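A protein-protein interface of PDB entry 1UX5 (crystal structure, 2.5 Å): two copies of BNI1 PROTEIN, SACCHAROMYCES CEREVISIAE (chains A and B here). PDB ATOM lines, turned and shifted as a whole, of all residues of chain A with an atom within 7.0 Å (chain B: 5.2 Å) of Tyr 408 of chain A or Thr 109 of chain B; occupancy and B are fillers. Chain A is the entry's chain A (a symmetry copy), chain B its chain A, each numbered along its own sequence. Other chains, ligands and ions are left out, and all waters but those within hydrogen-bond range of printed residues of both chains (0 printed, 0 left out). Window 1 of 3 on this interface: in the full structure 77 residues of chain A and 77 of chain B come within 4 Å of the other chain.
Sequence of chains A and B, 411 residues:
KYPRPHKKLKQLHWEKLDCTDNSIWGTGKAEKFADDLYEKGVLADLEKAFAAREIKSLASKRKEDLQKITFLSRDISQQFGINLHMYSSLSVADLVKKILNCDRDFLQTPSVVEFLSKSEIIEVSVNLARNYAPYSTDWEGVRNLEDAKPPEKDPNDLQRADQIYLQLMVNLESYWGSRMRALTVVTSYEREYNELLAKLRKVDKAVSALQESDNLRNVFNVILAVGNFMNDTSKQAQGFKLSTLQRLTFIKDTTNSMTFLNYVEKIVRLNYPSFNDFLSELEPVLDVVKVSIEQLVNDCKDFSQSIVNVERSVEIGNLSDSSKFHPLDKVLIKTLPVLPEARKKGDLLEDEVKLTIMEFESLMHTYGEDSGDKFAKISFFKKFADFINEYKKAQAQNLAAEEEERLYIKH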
ATOM      1  N   ALA A 401      21.492  24.970  37.686  1.00  0.00           N
ATOM      2  CA  ALA A 401      22.748  25.582  37.268  1.00  0.00           C
ATOM      3  C   ALA A 401      23.946  24.792  37.746  1.00  0.00           C
ATOM      4  O   ALA A 401      24.878  24.545  36.981  1.00  0.00           O
ATOM      5  CB  ALA A 401      22.840  27.000  37.792  1.00  0.00           C
ATOM      6  N   GLU A 403      24.204  21.652  38.451  1.00  0.00           N
ATOM      7  CA  GLU A 403      24.321  20.370  37.756  1.00  0.00           C
ATOM      8  C   GLU A 403      25.012  20.544  36.399  1.00  0.00           C
ATOM      9  O   GLU A 403      25.909  19.776  36.045  1.00  0.00           O
ATOM     10  CB  GLU A 403      22.940  19.757  37.552  1.00  0.00           C
ATOM     11  CG  GLU A 403      22.973  18.387  36.931  1.00  0.00           C
ATOM     12  CD  GLU A 403      21.600  17.928  36.495  1.00  0.00           C
ATOM     13  OE1 GLU A 403      20.694  17.867  37.351  1.00  0.00           O
ATOM     14  OE2 GLU A 403      21.427  17.633  35.294  1.00  0.00           O
ATOM     15  N   GLU A 404      24.583  21.553  35.646  1.00  0.00           N
ATOM     16  CA  GLU A 404      25.170  21.833  34.348  1.00  0.00           C
ATOM     17  C   GLU A 404      26.660  22.041  34.529  1.00  0.00           C
ATOM     18  O   GLU A 404      27.460  21.471  33.788  1.00  0.00           O
ATOM     19  CB  GLU A 404      24.560  23.086  33.732  1.00  0.00           C
ATOM     20  CG  GLU A 404      23.047  23.057  33.649  1.00  0.00           C
ATOM     21  CD  GLU A 404      22.481  24.253  32.901  1.00  0.00           C
ATOM     22  OE1 GLU A 404      21.255  24.478  32.990  1.00  0.00           O
ATOM     23  OE2 GLU A 404      23.260  24.960  32.220  1.00  0.00           O
ATOM     24  N   GLU A 405      27.037  22.855  35.511  1.00  0.00           N
ATOM     25  CA  GLU A 405      28.451  23.113  35.775  1.00  0.00           C
ATOM     26  C   GLU A 405      29.165  21.850  36.251  1.00  0.00           C
ATOM     27  O   GLU A 405      30.366  21.706  36.036  1.00  0.00           O
ATOM     28  CB  GLU A 405      28.622  24.219  36.821  1.00  0.00           C
ATOM     29  CG  GLU A 405      28.108  25.578  36.384  1.00  0.00           C
ATOM     30  CD  GLU A 405      28.283  26.643  37.455  1.00  0.00           C
ATOM     31  OE1 GLU A 405      27.690  26.501  38.547  1.00  0.00           O
ATOM     32  OE2 GLU A 405      29.015  27.624  37.201  1.00  0.00           O
ATOM     33  N   ARG A 406      28.439  20.942  36.903  1.00  0.00           N
ATOM     34  CA  ARG A 406      29.046  19.693  37.374  1.00  0.00           C
ATOM     35  C   ARG A 406      29.442  18.878  36.144  1.00  0.00           C
ATOM     36  O   ARG A 406      30.347  18.041  36.190  1.00  0.00           O
ATOM     37  CB  ARG A 406      28.061  18.883  38.229  1.00  0.00           C
ATOM     38  CG  ARG A 406      28.438  18.794  39.709  1.00  0.00           C
ATOM     39  CD  ARG A 406      27.567  17.789  40.485  1.00  0.00           C
ATOM     40  NE  ARG A 406      26.138  18.102  40.446  1.00  0.00           N
ATOM     41  CZ  ARG A 406      25.603  19.242  40.873  1.00  0.00           C
ATOM     42  NH1 ARG A 406      26.376  20.196  41.378  1.00  0.00           N
ATOM     43  NH2 ARG A 406      24.290  19.435  40.793  1.00  0.00           N
ATOM     44  N   LEU A 407      28.743  19.142  35.044  1.00  0.00           N
ATOM     45  CA  LEU A 407      28.980  18.470  33.780  1.00  0.00           C
ATOM     46  C   LEU A 407      30.139  19.154  33.072  1.00  0.00           C
ATOM     47  O   LEU A 407      31.220  18.587  32.935  1.00  0.00           O
ATOM     48  CB  LEU A 407      27.726  18.560  32.912  1.00  0.00           C
ATOM     49  CG  LEU A 407      27.703  17.712  31.643  1.00  0.00           C
ATOM     50  CD1 LEU A 407      27.881  16.249  32.026  1.00  0.00           C
ATOM     51  CD2 LEU A 407      26.387  17.916  30.902  1.00  0.00           C
ATOM     52  N   TYR A 408      29.898  20.387  32.637  1.00  0.00           N
ATOM     53  CA  TYR A 408      30.887  21.192  31.926  1.00  0.00           C
ATOM     54  C   TYR A 408      32.307  21.104  32.472  1.00  0.00           C
ATOM     55  O   TYR A 408      33.263  21.054  31.704  1.00  0.00           O
ATOM     56  CB  TYR A 408      30.432  22.653  31.894  1.00  0.00           C
ATOM     57  CG  TYR A 408      29.124  22.850  31.154  1.00  0.00           C
ATOM     58  CD1 TYR A 408      28.172  23.767  31.604  1.00  0.00           C
ATOM     59  CD2 TYR A 408      28.832  22.111  30.005  1.00  0.00           C
ATOM     60  CE1 TYR A 408      26.962  23.940  30.929  1.00  0.00           C
ATOM     61  CE2 TYR A 408      27.629  22.276  29.323  1.00  0.00           C
ATOM     62  CZ  TYR A 408      26.698  23.191  29.790  1.00  0.00           C
ATOM     63  OH  TYR A 408      25.505  23.348  29.120  1.00  0.00           O
ATOM     64  N   ILE A 409      32.451  21.079  33.792  1.00  0.00           N
ATOM     65  CA  ILE A 409      33.778  21.009  34.385  1.00  0.00           C
ATOM     66  C   ILE A 409      34.413  19.640  34.167  1.00  0.00           C
ATOM     67  O   ILE A 409      35.633  19.491  34.251  1.00  0.00           O
ATOM     68  CB  ILE A 409      33.732  21.344  35.890  1.00  0.00           C
ATOM     69  CG1 ILE A 409      33.257  22.789  36.075  1.00  0.00           C
ATOM     70  CG2 ILE A 409      35.109  21.173  36.509  1.00  0.00           C
ATOM     71  CD1 ILE A 409      33.162  23.239  37.519  1.00  0.00           C
ATOM     72  N   LYS A 410      33.581  18.647  33.867  1.00  0.00           N
ATOM     73  CA  LYS A 410      34.053  17.286  33.614  1.00  0.00           C
ATOM     74  C   LYS A 410      34.541  17.162  32.161  1.00  0.00           C
ATOM     75  O   LYS A 410      35.674  16.741  31.899  1.00  0.00           O
ATOM     76  CB  LYS A 410      32.913  16.302  33.883  1.00  0.00           C
ATOM     77  CG  LYS A 410      33.236  14.850  33.629  1.00  0.00           C
ATOM     78  CD  LYS A 410      31.998  14.007  33.884  1.00  0.00           C
ATOM     79  CE  LYS A 410      32.243  12.543  33.585  1.00  0.00           C
ATOM     80  NZ  LYS A 410      31.029  11.726  33.863  1.00  0.00           N
ATOM     81  N   HIS A 411      33.680  17.554  31.225  1.00  0.00           N
ATOM     82  CA  HIS A 411      33.996  17.501  29.801  1.00  0.00           C
ATOM     83  C   HIS A 411      34.626  18.812  29.324  1.00  0.00           C
ATOM     84  O   HIS A 411      35.834  19.015  29.446  1.00  0.00           O
ATOM     85  CB  HIS A 411      32.723  17.222  28.992  1.00  0.00           C
ATOM     86  CG  HIS A 411      31.952  16.027  29.465  1.00  0.00           C
ATOM     87  ND1 HIS A 411      32.533  14.791  29.659  1.00  0.00           N
ATOM     88  CD2 HIS A 411      30.642  15.878  29.776  1.00  0.00           C
ATOM     89  CE1 HIS A 411      31.615  13.934  30.070  1.00  0.00           C
ATOM     90  NE2 HIS A 411      30.458  14.568  30.150  1.00  0.00           N
ATOM     91  N   MET B  86      26.463  29.079  28.177  1.00  0.00           N
ATOM     92  CA  MET B  86      27.324  28.175  28.925  1.00  0.00           C
ATOM     93  C   MET B  86      28.724  28.138  28.331  1.00  0.00           C
ATOM     94  O   MET B  86      29.630  27.514  28.892  1.00  0.00           O
ATOM     95  CB  MET B  86      26.745  26.755  28.966  1.00  0.00           C
ATOM     96  CG  MET B  86      26.567  26.076  27.617  1.00  0.00           C
ATOM     97  SD  MET B  86      25.095  26.622  26.727  1.00  0.00           S
ATOM     98  CE  MET B  86      23.792  25.845  27.706  1.00  0.00           C
ATOM     99  N   TYR B  87      28.903  28.821  27.204  1.00  0.00           N
ATOM    100  CA  TYR B  87      30.201  28.848  26.544  1.00  0.00           C
ATOM    101  C   TYR B  87      30.775  30.264  26.463  1.00  0.00           C
ATOM    102  O   TYR B  87      31.718  30.529  25.711  1.00  0.00           O
ATOM    103  CB  TYR B  87      30.087  28.224  25.147  1.00  0.00           C
ATOM    104  CG  TYR B  87      29.657  26.768  25.168  1.00  0.00           C
ATOM    105  CD1 TYR B  87      28.402  26.378  24.691  1.00  0.00           C
ATOM    106  CD2 TYR B  87      30.495  25.782  25.694  1.00  0.00           C
ATOM    107  CE1 TYR B  87      27.991  25.037  24.741  1.00  0.00           C
ATOM    108  CE2 TYR B  87      30.095  24.438  25.749  1.00  0.00           C
ATOM    109  CZ  TYR B  87      28.844  24.074  25.273  1.00  0.00           C
ATOM    110  OH  TYR B  87      28.449  22.752  25.335  1.00  0.00           O
ATOM    111  N   ASP B 105      29.458  16.719  26.655  1.00  0.00           N
ATOM    112  CA  ASP B 105      28.590  17.685  27.333  1.00  0.00           C
ATOM    113  C   ASP B 105      27.733  18.441  26.317  1.00  0.00           C
ATOM    114  O   ASP B 105      26.568  18.746  26.569  1.00  0.00           O
ATOM    115  CB  ASP B 105      29.407  18.690  28.148  1.00  0.00           C
ATOM    116  CG  ASP B 105      30.293  19.568  27.279  1.00  0.00           C
ATOM    117  OD1 ASP B 105      31.333  19.061  26.811  1.00  0.00           O
ATOM    118  OD2 ASP B 105      29.948  20.756  27.063  1.00  0.00           O
ATOM    119  N   PHE B 106      28.326  18.747  25.168  1.00  0.00           N
ATOM    120  CA  PHE B 106      27.638  19.450  24.090  1.00  0.00           C
ATOM    121  C   PHE B 106      26.397  18.676  23.655  1.00  0.00           C
ATOM    122  O   PHE B 106      25.306  19.237  23.556  1.00  0.00           O
ATOM    123  CB  PHE B 106      28.600  19.621  22.910  1.00  0.00           C
ATOM    124  CG  PHE B 106      27.923  19.848  21.587  1.00  0.00           C
ATOM    125  CD1 PHE B 106      26.964  20.845  21.432  1.00  0.00           C
ATOM    126  CD2 PHE B 106      28.288  19.092  20.475  1.00  0.00           C
ATOM    127  CE1 PHE B 106      26.380  21.089  20.188  1.00  0.00           C
ATOM    128  CE2 PHE B 106      27.711  19.329  19.227  1.00  0.00           C
ATOM    129  CZ  PHE B 106      26.756  20.331  19.085  1.00  0.00           C
ATOM    130  N   LEU B 107      26.578  17.383  23.395  1.00  0.00           N
ATOM    131  CA  LEU B 107      25.485  16.517  22.970  1.00  0.00           C
ATOM    132  C   LEU B 107      24.443  16.371  24.074  1.00  0.00           C
ATOM    133  O   LEU B 107      23.243  16.357  23.805  1.00  0.00           O
ATOM    134  CB  LEU B 107      26.025  15.137  22.596  1.00  0.00           C
ATOM    135  CG  LEU B 107      27.046  15.060  21.456  1.00  0.00           C
ATOM    136  CD1 LEU B 107      27.716  13.689  21.463  1.00  0.00           C
ATOM    137  CD2 LEU B 107      26.362  15.324  20.124  1.00  0.00           C
ATOM    138  N   GLN B 108      24.900  16.261  25.318  1.00  0.00           N
ATOM    139  CA  GLN B 108      23.983  16.113  26.442  1.00  0.00           C
ATOM    140  C   GLN B 108      23.241  17.410  26.794  1.00  0.00           C
ATOM    141  O   GLN B 108      22.539  17.477  27.799  1.00  0.00           O
ATOM    142  CB  GLN B 108      24.735  15.561  27.661  1.00  0.00           C
ATOM    143  CG  GLN B 108      25.036  14.061  27.550  1.00  0.00           C
ATOM    144  CD  GLN B 108      25.957  13.532  28.651  1.00  0.00           C
ATOM    145  OE1 GLN B 108      25.755  13.806  29.836  1.00  0.00           O
ATOM    146  NE2 GLN B 108      26.963  12.753  28.258  1.00  0.00           N
ATOM    147  N   THR B 109      23.388  18.432  25.953  1.00  0.00           N
ATOM    148  CA  THR B 109      22.717  19.721  26.149  1.00  0.00           C
ATOM    149  C   THR B 109      21.677  19.884  25.028  1.00  0.00           C
ATOM    150  O   THR B 109      21.902  20.596  24.052  1.00  0.00           O
ATOM    151  CB  THR B 109      23.726  20.897  26.078  1.00  0.00           C
ATOM    152  OG1 THR B 109      24.780  20.690  27.028  1.00  0.00           O
ATOM    153  CG2 THR B 109      23.029  22.215  26.385  1.00  0.00           C
ATOM    154  N   PRO B 110      20.512  19.240  25.174  1.00  0.00           N
ATOM    155  CA  PRO B 110      19.411  19.270  24.203  1.00  0.00           C
ATOM    156  C   PRO B 110      19.087  20.628  23.589  1.00  0.00           C
ATOM    157  O   PRO B 110      18.736  20.714  22.408  1.00  0.00           O
ATOM    158  CB  PRO B 110      18.222  18.732  25.003  1.00  0.00           C
ATOM    159  CG  PRO B 110      18.871  17.850  26.020  1.00  0.00           C
ATOM    160  CD  PRO B 110      20.055  18.670  26.452  1.00  0.00           C
ATOM    161  N   SER B 111      19.196  21.682  24.396  1.00  0.00           N
ATOM    162  CA  SER B 111      18.861  23.029  23.946  1.00  0.00           C
ATOM    163  C   SER B 111      19.780  23.628  22.884  1.00  0.00           C
ATOM    164  O   SER B 111      19.322  24.385  22.024  1.00  0.00           O
ATOM    165  CB  SER B 111      18.783  23.978  25.146  1.00  0.00           C
ATOM    166  OG  SER B 111      20.041  24.114  25.781  1.00  0.00           O
ATOM    167  N   VAL B 112      21.069  23.308  22.939  1.00  0.00           N
ATOM    168  CA  VAL B 112      22.000  23.846  21.951  1.00  0.00           C
ATOM    169  C   VAL B 112      21.844  23.112  20.623  1.00  0.00           C
ATOM    170  O   VAL B 112      21.768  23.735  19.560  1.00  0.00           O
ATOM    171  CB  VAL B 112      23.470  23.731  22.424  1.00  0.00           C
ATOM    172  CG1 VAL B 112      23.646  24.470  23.735  1.00  0.00           C
ATOM    173  CG2 VAL B 112      23.861  22.277  22.583  1.00  0.00           C
ATOM    174  N   VAL B 113      21.784  21.786  20.695  1.00  0.00           N
ATOM    175  CA  VAL B 113      21.630  20.961  19.512  1.00  0.00           C
ATOM    176  C   VAL B 113      20.403  21.409  18.724  1.00  0.00           C
ATOM    177  O   VAL B 113      20.392  21.354  17.494  1.00  0.00           O
ATOM    178  CB  VAL B 113      21.495  19.485  19.904  1.00  0.00           C
ATOM    179  CG1 VAL B 113      21.330  18.612  18.659  1.00  0.00           C
ATOM    180  CG2 VAL B 113      22.721  19.066  20.696  1.00  0.00           C
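OE1 of Gln 108 of chain B touches CD1 of Leu 407 of chain A (3.9 Å).
Met 86 of chain B touches Tyr 408 of chain A (CG to OH, 3.3 Å).
CD2 of Tyr 408 of chain A touches OD2 of Asp 105 of chain B, at 3.4 Å.
CB of His 411 of chain A touches OD1 of Asp 105 of chain B (3.2 Å).
Tyr 408 of chain A touches just these residues of chain B: Met 86, Asp 105 and Thr 109.
Of chain A, only Tyr 408 comes within 4 Å of Thr 109 of chain B.
Of the printed residues of chain B, His 411 of chain A touches Asp 105.
Of the printed residues of chain B, Leu 407 of chain A touches Gln 108.
Ser 111 of chain B touches none of the printed residues of chain A.
Val 113 of chain B touches none of the printed residues of chain A.
The nearest residue of chain A that does not touch Thr 109 of chain B is Leu 407 of chain A (5.0 Å).
Along chain B the printed residues that touch a printed residue of chain A span positions 86 to 109.
Hydrophobic or aromatic side chains of chain A that line the printed part of chain B: Leu 407, Tyr 408 and His 411.
Among the printed residues, no Asp or Glu carboxylate lies within 4 Å of a Lys or Arg side-chain nitrogen of the other chain.
The side-chain hydroxyl of Thr 109 of chain B sits at hydrogen-bond distance from the side-chain hydroxyl of Tyr 408 of chain A (3.5 Å).
The backbone carbonyl oxygen (O) of Asp 105 of chain B is in hydrogen-bond range of the side-chain hydroxyl (OG1) of Thr 109 of chain B (2.7 Å).
The side-chain hydroxyl (OH) of Tyr 87 of chain B is in hydrogen-bond range of the side-chain carboxylate (OD2) of Asp 105 of chain B (3.0 Å).
No position is printed for both chains.
Of the 5 pairs that touch across the chains among the printed residues, none has its exchanged pair printed and touching as well.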
